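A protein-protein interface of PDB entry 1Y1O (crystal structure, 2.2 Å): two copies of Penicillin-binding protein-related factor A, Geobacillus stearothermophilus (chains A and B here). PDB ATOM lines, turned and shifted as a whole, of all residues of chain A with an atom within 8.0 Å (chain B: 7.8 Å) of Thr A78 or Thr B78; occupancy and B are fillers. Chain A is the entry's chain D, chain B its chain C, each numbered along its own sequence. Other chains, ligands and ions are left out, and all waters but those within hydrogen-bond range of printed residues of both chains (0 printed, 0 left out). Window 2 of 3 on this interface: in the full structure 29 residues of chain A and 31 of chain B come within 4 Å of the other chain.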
ATOM      1  N   ILE A  64       4.870 -20.178  -2.903  1.00  0.00           N
ATOM      2  CA  ILE A  64       4.721 -20.495  -1.495  1.00  0.00           C
ATOM      3  C   ILE A  64       4.243 -21.932  -1.400  1.00  0.00           C
ATOM      4  O   ILE A  64       3.189 -22.271  -1.962  1.00  0.00           O
ATOM      5  CB  ILE A  64       3.699 -19.563  -0.804  1.00  0.00           C
ATOM      6  CG1 ILE A  64       4.183 -18.110  -0.839  1.00  0.00           C
ATOM      7  CG2 ILE A  64       3.410 -20.036   0.617  1.00  0.00           C
ATOM      8  CD1 ILE A  64       3.072 -17.087  -0.900  1.00  0.00           C
ATOM      9  N   VAL A  65       5.031 -22.762  -0.711  1.00  0.00           N
ATOM     10  CA  VAL A  65       4.712 -24.178  -0.477  1.00  0.00           C
ATOM     11  C   VAL A  65       4.144 -24.389   0.933  1.00  0.00           C
ATOM     12  O   VAL A  65       3.005 -24.827   1.102  1.00  0.00           O
ATOM     13  CB  VAL A  65       5.940 -25.093  -0.652  1.00  0.00           C
ATOM     14  CG1 VAL A  65       5.519 -26.559  -0.630  1.00  0.00           C
ATOM     15  CG2 VAL A  65       6.682 -24.772  -1.932  1.00  0.00           C
ATOM     16  N   ARG A  66       4.935 -24.078   1.953  1.00  0.00           N
ATOM     17  CA  ARG A  66       4.473 -24.293   3.303  1.00  0.00           C
ATOM     18  C   ARG A  66       4.275 -22.989   4.049  1.00  0.00           C
ATOM     19  O   ARG A  66       5.052 -22.043   3.930  1.00  0.00           O
ATOM     20  CB  ARG A  66       5.417 -25.238   4.043  1.00  0.00           C
ATOM     21  CG  ARG A  66       5.324 -26.699   3.591  1.00  0.00           C
ATOM     22  CD  ARG A  66       6.490 -27.481   4.159  1.00  0.00           C
ATOM     23  NE  ARG A  66       6.105 -28.728   4.827  1.00  0.00           N
ATOM     24  CZ  ARG A  66       5.490 -28.795   6.012  1.00  0.00           C
ATOM     25  NH1 ARG A  66       5.152 -27.683   6.665  1.00  0.00           N
ATOM     26  NH2 ARG A  66       5.199 -29.976   6.540  1.00  0.00           N
ATOM     27  N   VAL A  67       3.184 -22.937   4.789  1.00  0.00           N
ATOM     28  CA  VAL A  67       2.912 -21.831   5.680  1.00  0.00           C
ATOM     29  C   VAL A  67       2.124 -22.372   6.864  1.00  0.00           C
ATOM     30  O   VAL A  67       1.296 -23.270   6.706  1.00  0.00           O
ATOM     31  CB  VAL A  67       2.209 -20.618   4.935  1.00  0.00           C
ATOM     32  CG1 VAL A  67       1.432 -21.081   3.717  1.00  0.00           C
ATOM     33  CG2 VAL A  67       1.340 -19.783   5.871  1.00  0.00           C
ATOM     34  N   ASP A  68       2.402 -21.871   8.056  1.00  0.00           N
ATOM     35  CA  ASP A  68       1.470 -22.124   9.130  1.00  0.00           C
ATOM     36  C   ASP A  68       0.789 -20.854   9.615  1.00  0.00           C
ATOM     37  O   ASP A  68       1.210 -19.738   9.300  1.00  0.00           O
ATOM     38  CB  ASP A  68       2.087 -22.956  10.265  1.00  0.00           C
ATOM     39  CG  ASP A  68       3.505 -22.561  10.575  1.00  0.00           C
ATOM     40  OD1 ASP A  68       3.732 -21.360  10.847  1.00  0.00           O
ATOM     41  OD2 ASP A  68       4.385 -23.454  10.554  1.00  0.00           O
ATOM     42  N   TYR A  69      -0.288 -21.049  10.366  1.00  0.00           N
ATOM     43  CA  TYR A  69      -1.202 -19.987  10.737  1.00  0.00           C
ATOM     44  C   TYR A  69      -1.456 -20.064  12.240  1.00  0.00           C
ATOM     45  O   TYR A  69      -2.441 -20.660  12.661  1.00  0.00           O
ATOM     46  CB  TYR A  69      -2.521 -20.136   9.948  1.00  0.00           C
ATOM     47  CG  TYR A  69      -2.328 -20.322   8.455  1.00  0.00           C
ATOM     48  CD1 TYR A  69      -2.114 -21.596   7.913  1.00  0.00           C
ATOM     49  CD2 TYR A  69      -2.357 -19.226   7.587  1.00  0.00           C
ATOM     50  CE1 TYR A  69      -1.923 -21.772   6.556  1.00  0.00           C
ATOM     51  CE2 TYR A  69      -2.168 -19.384   6.211  1.00  0.00           C
ATOM     52  CZ  TYR A  69      -1.953 -20.654   5.708  1.00  0.00           C
ATOM     53  OH  TYR A  69      -1.761 -20.832   4.366  1.00  0.00           O
ATOM     54  N   ALA A  75       0.766 -15.155   9.946  1.00  0.00           N
ATOM     55  CA  ALA A  75       1.023 -16.384   9.201  1.00  0.00           C
ATOM     56  C   ALA A  75       2.511 -16.375   8.831  1.00  0.00           C
ATOM     57  O   ALA A  75       3.072 -15.317   8.501  1.00  0.00           O
ATOM     58  CB  ALA A  75       0.142 -16.465   7.957  1.00  0.00           C
ATOM     59  N   VAL A  76       3.169 -17.532   8.935  1.00  0.00           N
ATOM     60  CA  VAL A  76       4.605 -17.600   8.642  1.00  0.00           C
ATOM     61  C   VAL A  76       4.871 -18.526   7.469  1.00  0.00           C
ATOM     62  O   VAL A  76       4.488 -19.704   7.484  1.00  0.00           O
ATOM     63  CB  VAL A  76       5.440 -18.072   9.859  1.00  0.00           C
ATOM     64  CG1 VAL A  76       6.900 -17.666   9.680  1.00  0.00           C
ATOM     65  CG2 VAL A  76       4.871 -17.503  11.163  1.00  0.00           C
ATOM     66  N   ILE A  77       5.526 -18.001   6.445  1.00  0.00           N
ATOM     67  CA  ILE A  77       5.943 -18.860   5.342  1.00  0.00           C
ATOM     68  C   ILE A  77       7.174 -19.641   5.772  1.00  0.00           C
ATOM     69  O   ILE A  77       8.182 -19.053   6.148  1.00  0.00           O
ATOM     70  CB  ILE A  77       6.255 -18.082   4.044  1.00  0.00           C
ATOM     71  CG1 ILE A  77       5.027 -17.291   3.594  1.00  0.00           C
ATOM     72  CG2 ILE A  77       6.761 -19.051   2.952  1.00  0.00           C
ATOM     73  CD1 ILE A  77       5.304 -16.293   2.485  1.00  0.00           C
ATOM     74  N   THR A  78       7.081 -20.960   5.704  1.00  0.00           N
ATOM     75  CA  THR A  78       8.162 -21.810   6.177  1.00  0.00           C
ATOM     76  C   THR A  78       8.903 -22.509   5.051  1.00  0.00           C
ATOM     77  O   THR A  78      10.040 -22.939   5.233  1.00  0.00           O
ATOM     78  CB  THR A  78       7.671 -22.820   7.249  1.00  0.00           C
ATOM     79  OG1 THR A  78       6.705 -23.715   6.674  1.00  0.00           O
ATOM     80  CG2 THR A  78       7.019 -22.065   8.383  1.00  0.00           C
ATOM     81  N   GLU A  79       8.259 -22.608   3.887  1.00  0.00           N
ATOM     82  CA  GLU A  79       8.896 -23.170   2.684  1.00  0.00           C
ATOM     83  C   GLU A  79       8.342 -22.446   1.454  1.00  0.00           C
ATOM     84  O   GLU A  79       7.128 -22.436   1.226  1.00  0.00           O
ATOM     85  CB  GLU A  79       8.640 -24.678   2.566  1.00  0.00           C
ATOM     86  CG  GLU A  79       9.681 -25.411   1.718  1.00  0.00           C
ATOM     87  CD  GLU A  79       9.286 -26.845   1.323  1.00  0.00           C
ATOM     88  OE1 GLU A  79       8.779 -27.627   2.178  1.00  0.00           O
ATOM     89  OE2 GLU A  79       9.522 -27.199   0.144  1.00  0.00           O
ATOM     90  N   ALA A  80       9.228 -21.810   0.697  1.00  0.00           N
ATOM     91  CA  ALA A  80       8.861 -21.121  -0.544  1.00  0.00           C
ATOM     92  C   ALA A  80      10.097 -21.021  -1.409  1.00  0.00           C
ATOM     93  O   ALA A  80      11.204 -21.009  -0.885  1.00  0.00           O
ATOM     94  CB  ALA A  80       8.274 -19.712  -0.269  1.00  0.00           C
ATOM     95  N   TYR A  81       9.903 -20.957  -2.723  1.00  0.00           N
ATOM     96  CA  TYR A  81      11.017 -20.856  -3.696  1.00  0.00           C
ATOM     97  C   TYR A  81      10.852 -19.604  -4.568  1.00  0.00           C
ATOM     98  O   TYR A  81       9.740 -19.109  -4.764  1.00  0.00           O
ATOM     99  CB  TYR A  81      11.130 -22.145  -4.544  1.00  0.00           C
ATOM    100  CG  TYR A  81      11.200 -23.372  -3.671  1.00  0.00           C
ATOM    101  CD1 TYR A  81      12.418 -23.782  -3.119  1.00  0.00           C
ATOM    102  CD2 TYR A  81      10.048 -24.090  -3.335  1.00  0.00           C
ATOM    103  CE1 TYR A  81      12.499 -24.885  -2.273  1.00  0.00           C
ATOM    104  CE2 TYR A  81      10.114 -25.192  -2.491  1.00  0.00           C
ATOM    105  CZ  TYR A  81      11.348 -25.584  -1.963  1.00  0.00           C
ATOM    106  OH  TYR A  81      11.451 -26.669  -1.122  1.00  0.00           O
ATOM    107  N   ILE B  64      10.895 -11.339   2.716  1.00  0.00           N
ATOM    108  CA  ILE B  64      11.829 -12.422   2.971  1.00  0.00           C
ATOM    109  C   ILE B  64      12.670 -12.115   4.213  1.00  0.00           C
ATOM    110  O   ILE B  64      13.216 -11.012   4.367  1.00  0.00           O
ATOM    111  CB  ILE B  64      12.707 -12.707   1.745  1.00  0.00           C
ATOM    112  CG1 ILE B  64      11.835 -13.240   0.617  1.00  0.00           C
ATOM    113  CG2 ILE B  64      13.811 -13.714   2.078  1.00  0.00           C
ATOM    114  CD1 ILE B  64      12.218 -12.692  -0.739  1.00  0.00           C
ATOM    115  N   VAL B  65      12.750 -13.094   5.106  1.00  0.00           N
ATOM    116  CA  VAL B  65      13.467 -12.914   6.360  1.00  0.00           C
ATOM    117  C   VAL B  65      14.655 -13.860   6.382  1.00  0.00           C
ATOM    118  O   VAL B  65      15.703 -13.510   6.893  1.00  0.00           O
ATOM    119  CB  VAL B  65      12.515 -13.076   7.600  1.00  0.00           C
ATOM    120  CG1 VAL B  65      13.278 -13.082   8.911  1.00  0.00           C
ATOM    121  CG2 VAL B  65      11.473 -11.956   7.617  1.00  0.00           C
ATOM    122  N   ARG B  66      14.501 -15.033   5.767  1.00  0.00           N
ATOM    123  CA  ARG B  66      15.506 -16.090   5.844  1.00  0.00           C
ATOM    124  C   ARG B  66      15.549 -16.985   4.593  1.00  0.00           C
ATOM    125  O   ARG B  66      14.550 -17.608   4.238  1.00  0.00           O
ATOM    126  CB  ARG B  66      15.219 -16.946   7.082  1.00  0.00           C
ATOM    127  CG  ARG B  66      16.324 -17.869   7.477  1.00  0.00           C
ATOM    128  CD  ARG B  66      16.966 -17.450   8.776  1.00  0.00           C
ATOM    129  NE  ARG B  66      17.858 -18.497   9.292  1.00  0.00           N
ATOM    130  CZ  ARG B  66      17.453 -19.673   9.780  1.00  0.00           C
ATOM    131  NH1 ARG B  66      16.149 -19.981   9.811  1.00  0.00           N
ATOM    132  NH2 ARG B  66      18.353 -20.547  10.238  1.00  0.00           N
ATOM    133  N   VAL B  67      16.715 -17.058   3.948  1.00  0.00           N
ATOM    134  CA  VAL B  67      16.953 -18.011   2.844  1.00  0.00           C
ATOM    135  C   VAL B  67      18.152 -18.933   3.120  1.00  0.00           C
ATOM    136  O   VAL B  67      19.162 -18.492   3.658  1.00  0.00           O
ATOM    137  CB  VAL B  67      17.136 -17.290   1.465  1.00  0.00           C
ATOM    138  CG1 VAL B  67      17.318 -18.313   0.308  1.00  0.00           C
ATOM    139  CG2 VAL B  67      15.967 -16.335   1.173  1.00  0.00           C
ATOM    140  N   ASP B  68      18.021 -20.201   2.723  1.00  0.00           N
ATOM    141  CA  ASP B  68      18.994 -21.277   2.987  1.00  0.00           C
ATOM    142  C   ASP B  68      19.522 -21.818   1.646  1.00  0.00           C
ATOM    143  O   ASP B  68      18.823 -21.736   0.631  1.00  0.00           O
ATOM    144  CB  ASP B  68      18.270 -22.378   3.789  1.00  0.00           C
ATOM    145  CG  ASP B  68      19.179 -23.523   4.252  1.00  0.00           C
ATOM    146  OD1 ASP B  68      20.432 -23.470   4.110  1.00  0.00           O
ATOM    147  OD2 ASP B  68      18.604 -24.505   4.790  1.00  0.00           O
ATOM    148  N   TYR B  69      20.748 -22.354   1.643  1.00  0.00           N
ATOM    149  CA  TYR B  69      21.383 -22.931   0.426  1.00  0.00           C
ATOM    150  C   TYR B  69      21.823 -24.398   0.526  1.00  0.00           C
ATOM    151  O   TYR B  69      22.860 -24.699   1.111  1.00  0.00           O
ATOM    152  CB  TYR B  69      22.552 -22.081  -0.023  1.00  0.00           C
ATOM    153  CG  TYR B  69      22.098 -20.879  -0.768  1.00  0.00           C
ATOM    154  CD1 TYR B  69      21.599 -19.776  -0.089  1.00  0.00           C
ATOM    155  CD2 TYR B  69      22.141 -20.842  -2.158  1.00  0.00           C
ATOM    156  CE1 TYR B  69      21.168 -18.664  -0.763  1.00  0.00           C
ATOM    157  CE2 TYR B  69      21.712 -19.726  -2.847  1.00  0.00           C
ATOM    158  CZ  TYR B  69      21.229 -18.634  -2.136  1.00  0.00           C
ATOM    159  OH  TYR B  69      20.792 -17.501  -2.788  1.00  0.00           O
ATOM    160  N   ALA B  75      17.740 -22.676  -3.985  1.00  0.00           N
ATOM    161  CA  ALA B  75      17.592 -21.862  -2.773  1.00  0.00           C
ATOM    162  C   ALA B  75      16.167 -21.903  -2.210  1.00  0.00           C
ATOM    163  O   ALA B  75      15.168 -21.859  -2.967  1.00  0.00           O
ATOM    164  CB  ALA B  75      18.030 -20.417  -3.035  1.00  0.00           C
ATOM    165  N   VAL B  76      16.089 -22.004  -0.881  1.00  0.00           N
ATOM    166  CA  VAL B  76      14.820 -22.131  -0.164  1.00  0.00           C
ATOM    167  C   VAL B  76      14.632 -20.966   0.792  1.00  0.00           C
ATOM    168  O   VAL B  76      15.508 -20.668   1.605  1.00  0.00           O
ATOM    169  CB  VAL B  76      14.738 -23.431   0.659  1.00  0.00           C
ATOM    170  CG1 VAL B  76      13.301 -23.703   1.084  1.00  0.00           C
ATOM    171  CG2 VAL B  76      15.288 -24.607  -0.122  1.00  0.00           C
ATOM    172  N   ILE B  77      13.492 -20.300   0.668  1.00  0.00           N
ATOM    173  CA  ILE B  77      13.068 -19.303   1.624  1.00  0.00           C
ATOM    174  C   ILE B  77      12.506 -20.099   2.810  1.00  0.00           C
ATOM    175  O   ILE B  77      11.552 -20.870   2.638  1.00  0.00           O
ATOM    176  CB  ILE B  77      12.004 -18.346   1.001  1.00  0.00           C
ATOM    177  CG1 ILE B  77      12.612 -17.566  -0.177  1.00  0.00           C
ATOM    178  CG2 ILE B  77      11.418 -17.417   2.055  1.00  0.00           C
ATOM    179  CD1 ILE B  77      11.594 -17.031  -1.176  1.00  0.00           C
ATOM    180  N   THR B  78      13.124 -19.948   3.989  1.00  0.00           N
ATOM    181  CA  THR B  78      12.704 -20.706   5.171  1.00  0.00           C
ATOM    182  C   THR B  78      11.871 -19.905   6.161  1.00  0.00           C
ATOM    183  O   THR B  78      11.249 -20.484   7.057  1.00  0.00           O
ATOM    184  CB  THR B  78      13.892 -21.322   5.946  1.00  0.00           C
ATOM    185  OG1 THR B  78      14.892 -20.317   6.180  1.00  0.00           O
ATOM    186  CG2 THR B  78      14.465 -22.515   5.197  1.00  0.00           C
ATOM    187  N   GLU B  79      11.881 -18.581   6.014  1.00  0.00           N
ATOM    188  CA  GLU B  79      11.028 -17.701   6.810  1.00  0.00           C
ATOM    189  C   GLU B  79      10.759 -16.460   6.007  1.00  0.00           C
ATOM    190  O   GLU B  79      11.657 -15.915   5.377  1.00  0.00           O
ATOM    191  CB  GLU B  79      11.653 -17.357   8.173  1.00  0.00           C
ATOM    192  CG  GLU B  79      10.797 -16.438   9.095  1.00  0.00           C
ATOM    193  CD  GLU B  79      11.567 -15.992  10.368  1.00  0.00           C
ATOM    194  OE1 GLU B  79      12.602 -16.613  10.731  1.00  0.00           O
ATOM    195  OE2 GLU B  79      11.122 -15.009  10.996  1.00  0.00           O
ATOM    196  N   ALA B  80       9.500 -16.039   6.012  1.00  0.00           N
ATOM    197  CA  ALA B  80       9.037 -14.946   5.175  1.00  0.00           C
ATOM    198  C   ALA B  80       7.631 -14.608   5.604  1.00  0.00           C
ATOM    199  O   ALA B  80       6.968 -15.445   6.197  1.00  0.00           O
ATOM    200  CB  ALA B  80       9.083 -15.346   3.697  1.00  0.00           C
ATOM    201  N   TYR B  81       7.187 -13.377   5.355  1.00  0.00           N
ATOM    202  CA  TYR B  81       5.875 -12.928   5.812  1.00  0.00           C
ATOM    203  C   TYR B  81       5.117 -12.279   4.668  1.00  0.00           C
ATOM    204  O   TYR B  81       5.735 -11.756   3.744  1.00  0.00           O
ATOM    205  CB  TYR B  81       5.998 -11.954   7.007  1.00  0.00           C
ATOM    206  CG  TYR B  81       6.630 -12.601   8.212  1.00  0.00           C
ATOM    207  CD1 TYR B  81       5.861 -13.307   9.150  1.00  0.00           C
ATOM    208  CD2 TYR B  81       8.006 -12.544   8.395  1.00  0.00           C
ATOM    209  CE1 TYR B  81       6.461 -13.928  10.250  1.00  0.00           C
ATOM    210  CE2 TYR B  81       8.604 -13.144   9.471  1.00  0.00           C
ATOM    211  CZ  TYR B  81       7.840 -13.830  10.402  1.00  0.00           C
ATOM    212  OH  TYR B  81       8.501 -14.432  11.450  1.00  0.00           O
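Among the printed residues, pairs that only touch across the chains: Ala A75 with Tyr B81, Val A76 with Ala B80, Val A76 with Tyr B81, Ile A77 with Thr B78, Ile A77 with Glu B79, Thr A78 with Ile B77, Glu A79 with Ile B77, Ala A80 with Val B76, Tyr A81 with Ala B75 and Tyr A81 with Val B76.
Of the 13 printed residues of chain B, 7 touch a printed residue of chain A. Hydrophobic or aromatic side chains of chain B that line the printed part of chain A: Val B76, Ile B77, Ala B80 and Tyr B81. Printed residues of chain A that touch a printed residue of chain B: Ala A75, Val A76, Ile A77, Thr A78, Glu A79, Ala A80 and Tyr A81.
Ala A75 touches Tyr B81, and with the chains exchanged Tyr A81 touches Ala B75. Ile A77 touches Thr B78, and with the chains exchanged Thr A78 touches Ile B77. Ile A77 touches Glu B79, and with the chains exchanged Glu A79 touches Ile B77. Thr B78 touches its own counterpart, Thr A78. Of the 13 pairs that touch across the chains among the printed residues, 13 have their exchanged pair printed and touching as well.
The backbone NH (N) of Val B65 is in hydrogen-bond range of the backbone carbonyl oxygen (O) of Glu B79, at 3.0 Å. The backbone NH of Thr B78 lies within hydrogen-bond range of the backbone carbonyl oxygen of Arg B66 (2.8 Å). N of Arg B66 lies within hydrogen-bond range of O of Glu B79 (3.0 Å). The backbone carbonyl oxygen of Val B76 lies within hydrogen-bond range of the backbone NH of Asp B68 (2.8 Å). The backbone carbonyl oxygen (O) of Arg A66 lies within hydrogen-bond range of the backbone NH (N) of Thr A78 (2.9 Å). The backbone carbonyl oxygen (O) of Asp A68 sits at hydrogen-bond distance from the backbone NH (N) of Val A76, 3.0 Å away.
O of Ala A80 is in hydrogen-bond range of N of Ile B77 (2.9 Å). O of Ala B80 lies within hydrogen-bond range of N of Ile A77 (2.9 Å). The backbone carbonyl oxygen of Thr B78 lies close to the backbone carbonyl oxygen of Thr A78 (3.3 Å).
Of the printed residues of chain B, Tyr A81 touches Ala B75 and Val B76. Of the printed residues of chain B, Ala A75 touches Tyr B81. Of the printed residues of chain B, Val A76 touches Ala B80 and Tyr B81. Printed residues of chain B within 4 Å of Ala A80: Val B76 (3.8 Å) and Ile B77 (2.9 Å). Val A65 touches none of the printed residues of chain B. Ile A64 touches none of the printed residues of chain B. The nearest residue of chain B that does not touch Thr A78 is Glu B79 (4.8 Å). The nearest residue of chain A that does not touch Thr B78 is Glu A79 (4.8 Å).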
